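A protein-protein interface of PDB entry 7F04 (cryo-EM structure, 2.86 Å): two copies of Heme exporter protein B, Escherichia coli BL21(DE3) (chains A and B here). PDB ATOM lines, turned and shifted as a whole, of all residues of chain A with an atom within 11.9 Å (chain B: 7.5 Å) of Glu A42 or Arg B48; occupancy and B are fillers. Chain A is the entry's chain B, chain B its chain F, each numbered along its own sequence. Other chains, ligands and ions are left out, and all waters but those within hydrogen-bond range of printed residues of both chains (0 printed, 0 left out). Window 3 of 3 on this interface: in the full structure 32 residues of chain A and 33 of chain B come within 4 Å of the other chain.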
ATOM      1  N   ILE A  32     -20.303   4.190  -7.458  1.00  0.00           N
ATOM      2  CA  ILE A  32     -20.687   3.481  -8.676  1.00  0.00           C
ATOM      3  C   ILE A  32     -22.171   3.671  -8.955  1.00  0.00           C
ATOM      4  O   ILE A  32     -22.576   3.920 -10.095  1.00  0.00           O
ATOM      5  CB  ILE A  32     -20.326   1.988  -8.566  1.00  0.00           C
ATOM      6  CG1 ILE A  32     -18.811   1.787  -8.503  1.00  0.00           C
ATOM      7  CG2 ILE A  32     -20.912   1.211  -9.732  1.00  0.00           C
ATOM      8  CD1 ILE A  32     -18.024   2.664  -9.429  1.00  0.00           C
ATOM      9  N   THR A  33     -23.004   3.557  -7.917  1.00  0.00           N
ATOM     10  CA  THR A  33     -24.447   3.693  -8.089  1.00  0.00           C
ATOM     11  C   THR A  33     -24.828   5.091  -8.560  1.00  0.00           C
ATOM     12  O   THR A  33     -25.840   5.262  -9.248  1.00  0.00           O
ATOM     13  CB  THR A  33     -25.150   3.358  -6.772  1.00  0.00           C
ATOM     14  OG1 THR A  33     -24.884   1.993  -6.428  1.00  0.00           O
ATOM     15  CG2 THR A  33     -26.653   3.547  -6.883  1.00  0.00           C
ATOM     16  N   LEU A  34     -24.027   6.099  -8.208  1.00  0.00           N
ATOM     17  CA  LEU A  34     -24.359   7.475  -8.573  1.00  0.00           C
ATOM     18  C   LEU A  34     -24.479   7.669 -10.081  1.00  0.00           C
ATOM     19  O   LEU A  34     -25.189   8.574 -10.530  1.00  0.00           O
ATOM     20  CB  LEU A  34     -23.309   8.434  -8.016  1.00  0.00           C
ATOM     21  CG  LEU A  34     -23.498   8.938  -6.588  1.00  0.00           C
ATOM     22  CD1 LEU A  34     -22.543  10.082  -6.322  1.00  0.00           C
ATOM     23  CD2 LEU A  34     -24.932   9.369  -6.353  1.00  0.00           C
ATOM     24  N   PHE A  35     -23.795   6.851 -10.875  1.00  0.00           N
ATOM     25  CA  PHE A  35     -23.707   7.082 -12.314  1.00  0.00           C
ATOM     26  C   PHE A  35     -24.930   6.599 -13.095  1.00  0.00           C
ATOM     27  O   PHE A  35     -25.382   7.313 -13.997  1.00  0.00           O
ATOM     28  CB  PHE A  35     -22.435   6.443 -12.873  1.00  0.00           C
ATOM     29  CG  PHE A  35     -21.210   7.286 -12.689  1.00  0.00           C
ATOM     30  CD1 PHE A  35     -20.523   7.278 -11.490  1.00  0.00           C
ATOM     31  CD2 PHE A  35     -20.753   8.096 -13.711  1.00  0.00           C
ATOM     32  CE1 PHE A  35     -19.398   8.052 -11.319  1.00  0.00           C
ATOM     33  CE2 PHE A  35     -19.628   8.872 -13.545  1.00  0.00           C
ATOM     34  CZ  PHE A  35     -18.949   8.849 -12.348  1.00  0.00           C
ATOM     35  N   PRO A  36     -25.478   5.407 -12.829  1.00  0.00           N
ATOM     36  CA  PRO A  36     -26.741   5.047 -13.492  1.00  0.00           C
ATOM     37  C   PRO A  36     -27.875   6.007 -13.195  1.00  0.00           C
ATOM     38  O   PRO A  36     -28.731   6.229 -14.060  1.00  0.00           O
ATOM     39  CB  PRO A  36     -27.035   3.646 -12.944  1.00  0.00           C
ATOM     40  CG  PRO A  36     -25.714   3.104 -12.608  1.00  0.00           C
ATOM     41  CD  PRO A  36     -24.919   4.256 -12.096  1.00  0.00           C
ATOM     42  N   LEU A  37     -27.912   6.583 -11.994  1.00  0.00           N
ATOM     43  CA  LEU A  37     -28.971   7.519 -11.640  1.00  0.00           C
ATOM     44  C   LEU A  37     -28.893   8.813 -12.434  1.00  0.00           C
ATOM     45  O   LEU A  37     -29.875   9.559 -12.476  1.00  0.00           O
ATOM     46  CB  LEU A  37     -28.914   7.824 -10.145  1.00  0.00           C
ATOM     47  CG  LEU A  37     -29.289   6.662  -9.231  1.00  0.00           C
ATOM     48  CD1 LEU A  37     -28.784   6.911  -7.825  1.00  0.00           C
ATOM     49  CD2 LEU A  37     -30.790   6.469  -9.236  1.00  0.00           C
ATOM     50  N   SER A  38     -27.753   9.098 -13.058  1.00  0.00           N
ATOM     51  CA  SER A  38     -27.564  10.314 -13.833  1.00  0.00           C
ATOM     52  C   SER A  38     -27.507  10.054 -15.329  1.00  0.00           C
ATOM     53  O   SER A  38     -28.234  10.692 -16.095  1.00  0.00           O
ATOM     54  CB  SER A  38     -26.285  11.024 -13.377  1.00  0.00           C
ATOM     55  OG  SER A  38     -25.171  10.154 -13.446  1.00  0.00           O
ATOM     56  N   ILE A  39     -26.652   9.131 -15.766  1.00  0.00           N
ATOM     57  CA  ILE A  39     -26.563   8.814 -17.188  1.00  0.00           C
ATOM     58  C   ILE A  39     -27.806   8.066 -17.650  1.00  0.00           C
ATOM     59  O   ILE A  39     -28.332   8.320 -18.740  1.00  0.00           O
ATOM     60  CB  ILE A  39     -25.282   8.013 -17.471  1.00  0.00           C
ATOM     61  CG1 ILE A  39     -24.093   8.640 -16.745  1.00  0.00           C
ATOM     62  CG2 ILE A  39     -25.018   7.949 -18.961  1.00  0.00           C
ATOM     63  CD1 ILE A  39     -23.657   9.959 -17.319  1.00  0.00           C
ATOM     64  N   GLY A  40     -28.294   7.134 -16.838  1.00  0.00           N
ATOM     65  CA  GLY A  40     -29.410   6.301 -17.209  1.00  0.00           C
ATOM     66  C   GLY A  40     -29.153   4.851 -16.861  1.00  0.00           C
ATOM     67  O   GLY A  40     -28.041   4.469 -16.483  1.00  0.00           O
ATOM     68  N   PRO A  41     -30.176   4.008 -16.982  1.00  0.00           N
ATOM     69  CA  PRO A  41     -30.036   2.595 -16.616  1.00  0.00           C
ATOM     70  C   PRO A  41     -29.611   1.672 -17.748  1.00  0.00           C
ATOM     71  O   PRO A  41     -29.498   0.464 -17.515  1.00  0.00           O
ATOM     72  CB  PRO A  41     -31.452   2.242 -16.145  1.00  0.00           C
ATOM     73  CG  PRO A  41     -32.352   3.154 -16.926  1.00  0.00           C
ATOM     74  CD  PRO A  41     -31.539   4.319 -17.438  1.00  0.00           C
ATOM     75  N   GLU A  42     -29.378   2.194 -18.948  1.00  0.00           N
ATOM     76  CA  GLU A  42     -29.003   1.341 -20.071  1.00  0.00           C
ATOM     77  C   GLU A  42     -27.648   0.699 -19.801  1.00  0.00           C
ATOM     78  O   GLU A  42     -26.697   1.400 -19.439  1.00  0.00           O
ATOM     79  CB  GLU A  42     -28.955   2.145 -21.367  1.00  0.00           C
ATOM     80  CG  GLU A  42     -28.550   1.328 -22.581  1.00  0.00           C
ATOM     81  CD  GLU A  42     -28.103   2.188 -23.744  1.00  0.00           C
ATOM     82  OE1 GLU A  42     -27.790   3.376 -23.522  1.00  0.00           O
ATOM     83  OE2 GLU A  42     -28.061   1.674 -24.880  1.00  0.00           O
ATOM     84  N   PRO A  43     -27.515  -0.621 -19.964  1.00  0.00           N
ATOM     85  CA  PRO A  43     -26.245  -1.274 -19.626  1.00  0.00           C
ATOM     86  C   PRO A  43     -25.171  -1.128 -20.686  1.00  0.00           C
ATOM     87  O   PRO A  43     -23.984  -1.241 -20.351  1.00  0.00           O
ATOM     88  CB  PRO A  43     -26.645  -2.743 -19.451  1.00  0.00           C
ATOM     89  CG  PRO A  43     -27.826  -2.912 -20.343  1.00  0.00           C
ATOM     90  CD  PRO A  43     -28.520  -1.579 -20.454  1.00  0.00           C
ATOM     91  N   GLN A  44     -25.539  -0.897 -21.948  1.00  0.00           N
ATOM     92  CA  GLN A  44     -24.527  -0.728 -22.986  1.00  0.00           C
ATOM     93  C   GLN A  44     -23.758   0.573 -22.804  1.00  0.00           C
ATOM     94  O   GLN A  44     -22.537   0.609 -22.991  1.00  0.00           O
ATOM     95  CB  GLN A  44     -25.175  -0.778 -24.367  1.00  0.00           C
ATOM     96  CG  GLN A  44     -24.182  -0.699 -25.511  1.00  0.00           C
ATOM     97  CD  GLN A  44     -24.822  -0.943 -26.861  1.00  0.00           C
ATOM     98  OE1 GLN A  44     -26.045  -1.023 -26.976  1.00  0.00           O
ATOM     99  NE2 GLN A  44     -23.997  -1.070 -27.892  1.00  0.00           N
ATOM    100  N   LEU A  45     -24.455   1.654 -22.449  1.00  0.00           N
ATOM    101  CA  LEU A  45     -23.774   2.926 -22.234  1.00  0.00           C
ATOM    102  C   LEU A  45     -22.953   2.914 -20.953  1.00  0.00           C
ATOM    103  O   LEU A  45     -21.908   3.567 -20.885  1.00  0.00           O
ATOM    104  CB  LEU A  45     -24.784   4.071 -22.206  1.00  0.00           C
ATOM    105  CG  LEU A  45     -24.177   5.474 -22.158  1.00  0.00           C
ATOM    106  CD1 LEU A  45     -23.091   5.625 -23.211  1.00  0.00           C
ATOM    107  CD2 LEU A  45     -25.247   6.535 -22.336  1.00  0.00           C
ATOM    108  N   LEU A  46     -23.410   2.195 -19.927  1.00  0.00           N
ATOM    109  CA  LEU A  46     -22.632   2.088 -18.699  1.00  0.00           C
ATOM    110  C   LEU A  46     -21.323   1.344 -18.929  1.00  0.00           C
ATOM    111  O   LEU A  46     -20.355   1.556 -18.192  1.00  0.00           O
ATOM    112  CB  LEU A  46     -23.446   1.390 -17.613  1.00  0.00           C
ATOM    113  CG  LEU A  46     -24.523   2.214 -16.908  1.00  0.00           C
ATOM    114  CD1 LEU A  46     -25.211   1.376 -15.850  1.00  0.00           C
ATOM    115  CD2 LEU A  46     -23.927   3.466 -16.297  1.00  0.00           C
ATOM    116  N   ALA A  47     -21.278   0.465 -19.932  1.00  0.00           N
ATOM    117  CA  ALA A  47     -20.044  -0.253 -20.230  1.00  0.00           C
ATOM    118  C   ALA A  47     -19.028   0.651 -20.916  1.00  0.00           C
ATOM    119  O   ALA A  47     -17.837   0.616 -20.588  1.00  0.00           O
ATOM    120  CB  ALA A  47     -20.347  -1.476 -21.091  1.00  0.00           C
ATOM    121  N   ARG A  48     -19.475   1.463 -21.877  1.00  0.00           N
ATOM    122  CA  ARG A  48     -18.576   2.405 -22.530  1.00  0.00           C
ATOM    123  C   ARG A  48     -18.127   3.511 -21.586  1.00  0.00           C
ATOM    124  O   ARG A  48     -17.065   4.104 -21.799  1.00  0.00           O
ATOM    125  CB  ARG A  48     -19.248   3.010 -23.764  1.00  0.00           C
ATOM    126  CG  ARG A  48     -18.310   3.825 -24.642  1.00  0.00           C
ATOM    127  CD  ARG A  48     -18.954   4.225 -25.956  1.00  0.00           C
ATOM    128  NE  ARG A  48     -18.859   3.176 -26.963  1.00  0.00           N
ATOM    129  CZ  ARG A  48     -19.898   2.528 -27.473  1.00  0.00           C
ATOM    130  NH1 ARG A  48     -21.137   2.797 -27.093  1.00  0.00           N
ATOM    131  NH2 ARG A  48     -19.689   1.587 -28.389  1.00  0.00           N
ATOM    132  N   ILE A  49     -18.909   3.791 -20.544  1.00  0.00           N
ATOM    133  CA  ILE A  49     -18.564   4.818 -19.568  1.00  0.00           C
ATOM    134  C   ILE A  49     -17.756   4.237 -18.413  1.00  0.00           C
ATOM    135  O   ILE A  49     -17.124   4.994 -17.661  1.00  0.00           O
ATOM    136  CB  ILE A  49     -19.882   5.491 -19.123  1.00  0.00           C
ATOM    137  CG1 ILE A  49     -20.392   6.416 -20.222  1.00  0.00           C
ATOM    138  CG2 ILE A  49     -19.712   6.343 -17.890  1.00  0.00           C
ATOM    139  CD1 ILE A  49     -19.368   7.401 -20.691  1.00  0.00           C
ATOM    140  N   ALA A  50     -17.696   2.909 -18.300  1.00  0.00           N
ATOM    141  CA  ALA A  50     -17.139   2.264 -17.113  1.00  0.00           C
ATOM    142  C   ALA A  50     -15.706   2.659 -16.770  1.00  0.00           C
ATOM    143  O   ALA A  50     -15.424   2.833 -15.571  1.00  0.00           O
ATOM    144  CB  ALA A  50     -17.248   0.741 -17.266  1.00  0.00           C
ATOM    145  N   ILE A  53     -15.916   5.880 -14.896  1.00  0.00           N
ATOM    146  CA  ILE A  53     -16.543   5.704 -13.587  1.00  0.00           C
ATOM    147  C   ILE A  53     -15.536   5.153 -12.592  1.00  0.00           C
ATOM    148  O   ILE A  53     -15.355   5.690 -11.489  1.00  0.00           O
ATOM    149  CB  ILE A  53     -17.765   4.776 -13.699  1.00  0.00           C
ATOM    150  CG1 ILE A  53     -18.793   5.337 -14.671  1.00  0.00           C
ATOM    151  CG2 ILE A  53     -18.401   4.577 -12.347  1.00  0.00           C
ATOM    152  CD1 ILE A  53     -19.963   4.411 -14.889  1.00  0.00           C
ATOM    153  N   VAL A 115     -18.159  -4.826  -9.094  1.00  0.00           N
ATOM    154  CA  VAL A 115     -18.435  -3.646  -9.911  1.00  0.00           C
ATOM    155  C   VAL A 115     -18.145  -3.871 -11.383  1.00  0.00           C
ATOM    156  O   VAL A 115     -18.431  -2.988 -12.202  1.00  0.00           O
ATOM    157  CB  VAL A 115     -17.633  -2.420  -9.431  1.00  0.00           C
ATOM    158  CG1 VAL A 115     -17.997  -2.078  -7.996  1.00  0.00           C
ATOM    159  CG2 VAL A 115     -16.151  -2.678  -9.560  1.00  0.00           C
ATOM    160  N   MET A 117     -19.671  -6.264 -12.970  1.00  0.00           N
ATOM    161  CA  MET A 117     -20.935  -6.758 -13.489  1.00  0.00           C
ATOM    162  C   MET A 117     -22.097  -5.809 -13.259  1.00  0.00           C
ATOM    163  O   MET A 117     -23.103  -5.917 -13.967  1.00  0.00           O
ATOM    164  CB  MET A 117     -21.261  -8.138 -12.888  1.00  0.00           C
ATOM    165  CG  MET A 117     -21.425  -8.200 -11.375  1.00  0.00           C
ATOM    166  SD  MET A 117     -23.020  -7.634 -10.749  1.00  0.00           S
ATOM    167  CE  MET A 117     -24.088  -8.959 -11.301  1.00  0.00           C
ATOM    168  N   LEU A 118     -21.996  -4.889 -12.295  1.00  0.00           N
ATOM    169  CA  LEU A 118     -22.962  -3.798 -12.221  1.00  0.00           C
ATOM    170  C   LEU A 118     -22.895  -2.932 -13.469  1.00  0.00           C
ATOM    171  O   LEU A 118     -23.930  -2.544 -14.022  1.00  0.00           O
ATOM    172  CB  LEU A 118     -22.712  -2.948 -10.976  1.00  0.00           C
ATOM    173  CG  LEU A 118     -23.514  -3.255  -9.712  1.00  0.00           C
ATOM    174  CD1 LEU A 118     -23.091  -4.568  -9.109  1.00  0.00           C
ATOM    175  CD2 LEU A 118     -23.349  -2.130  -8.705  1.00  0.00           C
ATOM    176  N   LEU A 119     -21.682  -2.613 -13.922  1.00  0.00           N
ATOM    177  CA  LEU A 119     -21.517  -1.808 -15.122  1.00  0.00           C
ATOM    178  C   LEU A 119     -21.739  -2.619 -16.393  1.00  0.00           C
ATOM    179  O   LEU A 119     -22.290  -2.094 -17.366  1.00  0.00           O
ATOM    180  CB  LEU A 119     -20.131  -1.165 -15.123  1.00  0.00           C
ATOM    181  CG  LEU A 119     -19.883  -0.277 -13.901  1.00  0.00           C
ATOM    182  CD1 LEU A 119     -18.456   0.235 -13.858  1.00  0.00           C
ATOM    183  CD2 LEU A 119     -20.868   0.878 -13.877  1.00  0.00           C
ATOM    184  N   GLY A 120     -21.337  -3.879 -16.404  1.00  0.00           N
ATOM    185  CA  GLY A 120     -21.568  -4.754 -17.528  1.00  0.00           C
ATOM    186  C   GLY A 120     -20.340  -5.211 -18.295  1.00  0.00           C
ATOM    187  O   GLY A 120     -20.465  -5.530 -19.484  1.00  0.00           O
ATOM    188  N   MET A 121     -19.173  -5.252 -17.665  1.00  0.00           N
ATOM    189  CA  MET A 121     -17.964  -5.672 -18.350  1.00  0.00           C
ATOM    190  C   MET A 121     -17.855  -7.194 -18.374  1.00  0.00           C
ATOM    191  O   MET A 121     -18.461  -7.902 -17.566  1.00  0.00           O
ATOM    192  CB  MET A 121     -16.736  -5.063 -17.675  1.00  0.00           C
ATOM    193  CG  MET A 121     -16.662  -3.556 -17.809  1.00  0.00           C
ATOM    194  SD  MET A 121     -15.182  -2.863 -17.060  1.00  0.00           S
ATOM    195  CE  MET A 121     -15.616  -3.020 -15.337  1.00  0.00           C
ATOM    196  N   GLU B  42     -17.712  11.203 -31.130  1.00  0.00           N
ATOM    197  CA  GLU B  42     -19.103  10.752 -31.103  1.00  0.00           C
ATOM    198  C   GLU B  42     -19.935  11.851 -30.460  1.00  0.00           C
ATOM    199  O   GLU B  42     -20.199  11.819 -29.252  1.00  0.00           O
ATOM    200  CB  GLU B  42     -19.248   9.431 -30.346  1.00  0.00           C
ATOM    201  CG  GLU B  42     -18.589   8.247 -31.027  1.00  0.00           C
ATOM    202  CD  GLU B  42     -18.839   6.947 -30.292  1.00  0.00           C
ATOM    203  OE1 GLU B  42     -19.450   6.988 -29.203  1.00  0.00           O
ATOM    204  OE2 GLU B  42     -18.426   5.884 -30.801  1.00  0.00           O
ATOM    205  N   PRO B  43     -20.340  12.858 -31.237  1.00  0.00           N
ATOM    206  CA  PRO B  43     -21.150  13.945 -30.662  1.00  0.00           C
ATOM    207  C   PRO B  43     -22.468  13.474 -30.079  1.00  0.00           C
ATOM    208  O   PRO B  43     -22.927  14.033 -29.076  1.00  0.00           O
ATOM    209  CB  PRO B  43     -21.369  14.889 -31.853  1.00  0.00           C
ATOM    210  CG  PRO B  43     -20.349  14.496 -32.868  1.00  0.00           C
ATOM    211  CD  PRO B  43     -20.117  13.036 -32.679  1.00  0.00           C
ATOM    212  N   GLN B  44     -23.094  12.461 -30.681  1.00  0.00           N
ATOM    213  CA  GLN B  44     -24.373  11.971 -30.179  1.00  0.00           C
ATOM    214  C   GLN B  44     -24.227  11.352 -28.795  1.00  0.00           C
ATOM    215  O   GLN B  44     -25.067  11.577 -27.917  1.00  0.00           O
ATOM    216  CB  GLN B  44     -24.964  10.956 -31.155  1.00  0.00           C
ATOM    217  CG  GLN B  44     -25.043  11.443 -32.590  1.00  0.00           C
ATOM    218  CD  GLN B  44     -23.854  11.002 -33.420  1.00  0.00           C
ATOM    219  OE1 GLN B  44     -23.153  10.053 -33.066  1.00  0.00           O
ATOM    220  NE2 GLN B  44     -23.623  11.687 -34.534  1.00  0.00           N
ATOM    221  N   LEU B  45     -23.175  10.561 -28.584  1.00  0.00           N
ATOM    222  CA  LEU B  45     -23.002   9.900 -27.296  1.00  0.00           C
ATOM    223  C   LEU B  45     -22.530  10.874 -26.227  1.00  0.00           C
ATOM    224  O   LEU B  45     -22.820  10.677 -25.042  1.00  0.00           O
ATOM    225  CB  LEU B  45     -22.022   8.735 -27.436  1.00  0.00           C
ATOM    226  CG  LEU B  45     -21.986   7.703 -26.310  1.00  0.00           C
ATOM    227  CD1 LEU B  45     -21.788   6.319 -26.894  1.00  0.00           C
ATOM    228  CD2 LEU B  45     -20.888   8.017 -25.309  1.00  0.00           C
ATOM    229  N   LEU B  46     -21.797  11.918 -26.619  1.00  0.00           N
ATOM    230  CA  LEU B  46     -21.392  12.942 -25.661  1.00  0.00           C
ATOM    231  C   LEU B  46     -22.598  13.695 -25.117  1.00  0.00           C
ATOM    232  O   LEU B  46     -22.663  13.998 -23.920  1.00  0.00           O
ATOM    233  CB  LEU B  46     -20.409  13.911 -26.315  1.00  0.00           C
ATOM    234  CG  LEU B  46     -20.176  15.241 -25.595  1.00  0.00           C
ATOM    235  CD1 LEU B  46     -19.310  15.042 -24.362  1.00  0.00           C
ATOM    236  CD2 LEU B  46     -19.553  16.262 -26.533  1.00  0.00           C
ATOM    237  N   ALA B  47     -23.562  14.012 -25.985  1.00  0.00           N
ATOM    238  CA  ALA B  47     -24.736  14.758 -25.556  1.00  0.00           C
ATOM    239  C   ALA B  47     -25.584  13.966 -24.570  1.00  0.00           C
ATOM    240  O   ALA B  47     -26.257  14.558 -23.719  1.00  0.00           O
ATOM    241  CB  ALA B  47     -25.572  15.157 -26.769  1.00  0.00           C
ATOM    242  N   ARG B  48     -25.570  12.638 -24.668  1.00  0.00           N
ATOM    243  CA  ARG B  48     -26.370  11.817 -23.768  1.00  0.00           C
ATOM    244  C   ARG B  48     -25.754  11.728 -22.378  1.00  0.00           C
ATOM    245  O   ARG B  48     -26.484  11.645 -21.386  1.00  0.00           O
ATOM    246  CB  ARG B  48     -26.554  10.421 -24.365  1.00  0.00           C
ATOM    247  CG  ARG B  48     -27.357   9.461 -23.504  1.00  0.00           C
ATOM    248  CD  ARG B  48     -28.343   8.675 -24.352  1.00  0.00           C
ATOM    249  NE  ARG B  48     -27.683   7.968 -25.444  1.00  0.00           N
ATOM    250  CZ  ARG B  48     -27.386   6.676 -25.433  1.00  0.00           C
ATOM    251  NH1 ARG B  48     -27.705   5.902 -24.410  1.00  0.00           N
ATOM    252  NH2 ARG B  48     -26.757   6.147 -26.478  1.00  0.00           N
ATOM    253  N   ILE B  49     -24.424  11.756 -22.283  1.00  0.00           N
ATOM    254  CA  ILE B  49     -23.745  11.608 -21.000  1.00  0.00           C
ATOM    255  C   ILE B  49     -23.326  12.935 -20.391  1.00  0.00           C
ATOM    256  O   ILE B  49     -22.883  12.953 -19.232  1.00  0.00           O
ATOM    257  CB  ILE B  49     -22.506  10.695 -21.124  1.00  0.00           C
ATOM    258  CG1 ILE B  49     -21.378  11.435 -21.840  1.00  0.00           C
ATOM    259  CG2 ILE B  49     -22.854   9.416 -21.860  1.00  0.00           C
ATOM    260  CD1 ILE B  49     -20.006  10.864 -21.580  1.00  0.00           C
ATOM    261  N   ALA B  50     -23.442  14.042 -21.126  1.00  0.00           N
ATOM    262  CA  ALA B  50     -22.964  15.324 -20.609  1.00  0.00           C
ATOM    263  C   ALA B  50     -23.673  15.763 -19.334  1.00  0.00           C
ATOM    264  O   ALA B  50     -22.977  16.083 -18.354  1.00  0.00           O
ATOM    265  CB  ALA B  50     -23.069  16.389 -21.707  1.00  0.00           C
ATOM    266  N   PRO B  51     -25.011  15.814 -19.260  1.00  0.00           N
ATOM    267  CA  PRO B  51     -25.635  16.231 -17.993  1.00  0.00           C
ATOM    268  C   PRO B  51     -25.278  15.335 -16.825  1.00  0.00           C
ATOM    269  O   PRO B  51     -25.026  15.825 -15.714  1.00  0.00           O
ATOM    270  CB  PRO B  51     -27.135  16.171 -18.311  1.00  0.00           C
ATOM    271  CG  PRO B  51     -27.220  16.248 -19.784  1.00  0.00           C
ATOM    272  CD  PRO B  51     -26.031  15.508 -20.277  1.00  0.00           C
ATOM    273  N   GLY B  52     -25.239  14.023 -17.055  1.00  0.00           N
ATOM    274  CA  GLY B  52     -24.965  13.103 -15.966  1.00  0.00           C
ATOM    275  C   GLY B  52     -23.572  13.277 -15.400  1.00  0.00           C
ATOM    276  O   GLY B  52     -23.389  13.344 -14.185  1.00  0.00           O
ATOM    277  N   ILE B  53     -22.569  13.360 -16.277  1.00  0.00           N
ATOM    278  CA  ILE B  53     -21.203  13.529 -15.799  1.00  0.00           C
ATOM    279  C   ILE B  53     -21.027  14.905 -15.173  1.00  0.00           C
ATOM    280  O   ILE B  53     -20.307  15.054 -14.181  1.00  0.00           O
ATOM    281  CB  ILE B  53     -20.185  13.272 -16.925  1.00  0.00           C
ATOM    282  CG1 ILE B  53     -20.295  14.322 -18.030  1.00  0.00           C
ATOM    283  CG2 ILE B  53     -20.355  11.869 -17.485  1.00  0.00           C
ATOM    284  CD1 ILE B  53     -19.009  14.537 -18.788  1.00  0.00           C
ATOM    285  N   ASP B 181     -31.185  17.185 -19.225  1.00  0.00           N
ATOM    286  CA  ASP B 181     -31.459  16.336 -20.377  1.00  0.00           C
ATOM    287  C   ASP B 181     -32.645  16.853 -21.176  1.00  0.00           C
ATOM    288  O   ASP B 181     -32.594  16.898 -22.409  1.00  0.00           O
ATOM    289  CB  ASP B 181     -31.703  14.900 -19.917  1.00  0.00           C
ATOM    290  CG  ASP B 181     -31.645  13.903 -21.058  1.00  0.00           C
ATOM    291  OD1 ASP B 181     -30.529  13.604 -21.533  1.00  0.00           O
ATOM    292  OD2 ASP B 181     -32.717  13.416 -21.478  1.00  0.00           O
ATOM    293  N   SER B 184     -31.769  19.518 -23.526  1.00  0.00           N
ATOM    294  CA  SER B 184     -31.139  19.125 -24.782  1.00  0.00           C
ATOM    295  C   SER B 184     -32.165  18.997 -25.899  1.00  0.00           C
ATOM    296  O   SER B 184     -31.910  19.413 -27.034  1.00  0.00           O
ATOM    297  CB  SER B 184     -30.381  17.812 -24.601  1.00  0.00           C
ATOM    298  OG  SER B 184     -29.613  17.829 -23.412  1.00  0.00           O
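Of the 14 printed residues of chain B, 5 touch a printed residue of chain A.
Of the 26 printed residues of chain A, 6 touch a printed residue of chain B.
Hydrophobic or aromatic side chains of chain A that line the printed part of chain B: Ile A39, Leu A45 and Ile A49.
Among the printed residues, Asp or Glu carboxylates within 4 Å of a Lys or Arg side-chain nitrogen of the other chain: Glu A42 with Arg B48.
Glu A42 touches Arg B48, but with the chains exchanged Arg A48 does not touch Glu B42 (4.3 Å).
Leu A45 touches Arg B48, and with the chains exchanged Arg A48 touches Leu B45.
Leu A45 touches Ile B49, but with the chains exchanged Ile A49 does not touch Leu B45 (4.9 Å).
Ile A49 touches its own counterpart, Ile B49.
Of the 10 pairs that touch across the chains among the printed residues, 4 have their exchanged pair printed and touching as well.
O of Leu A34 sits at hydrogen-bond distance from OG of Ser A38, 3.3 Å away.
The backbone carbonyl oxygen (O) of Phe A35 is in hydrogen-bond range of the side-chain hydroxyl (OG) of Ser A38 (2.9 Å).
Ser A38 touches Gly B52 (CB to CA, 3.6 Å).
Ile B49 touches Ile A39.
Gly B52 touches Ile A39.
Ile A39 touches Ile B53.
Leu A45 touches Leu B45.
NH1 of Arg B48 touches CD2 of Leu A45 (3.3 Å).
Leu A45 touches Ile B49.
Arg A48 touches Leu B45.
CD1 of Ile A49 touches CD1 of Ile B49, 3.6 Å away.
Printed residues of chain B within 4 Å of Ser A38: Gly B52.
Of the printed residues of chain B, Ile A39 touches Ile B49 (3.6 Å), Gly B52 (3.7 Å) and Ile B53 (3.7 Å).
Of chain B, only Arg B48 comes within 4 Å of Glu A42.
Printed residues of chain B within 4 Å of Leu A45: Leu B45 (3.9 Å), Arg B48 (3.3 Å) and Ile B49 (3.8 Å).
Ala A47 touches none of the printed residues of chain B.
Of the printed residues of chain B, Arg A48 touches Leu B45.
Of chain A, only Leu A45 (3.9 Å) and Arg A48 (3.6 Å) come within 4 Å of Leu B45.
Leu B46 touches none of the printed residues of chain A.
Of the printed residues of chain A, Arg B48 touches Glu A42 and Leu A45.
Ile B49 touches three residues of chain A.
No residue of chain A comes within 4 Å of Ala B50.
No residue of chain A comes within 4 Å of Pro B51.
Of the printed residues of chain A, Gly B52 touches Ser A38 and Ile A39.
The nearest printed residue of chain B that does not touch Glu A42 is Leu B45 (7.5 Å).
OE1 of Glu A42 is in salt-bridge range of NH1 of Arg B48 (2.7 Å).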
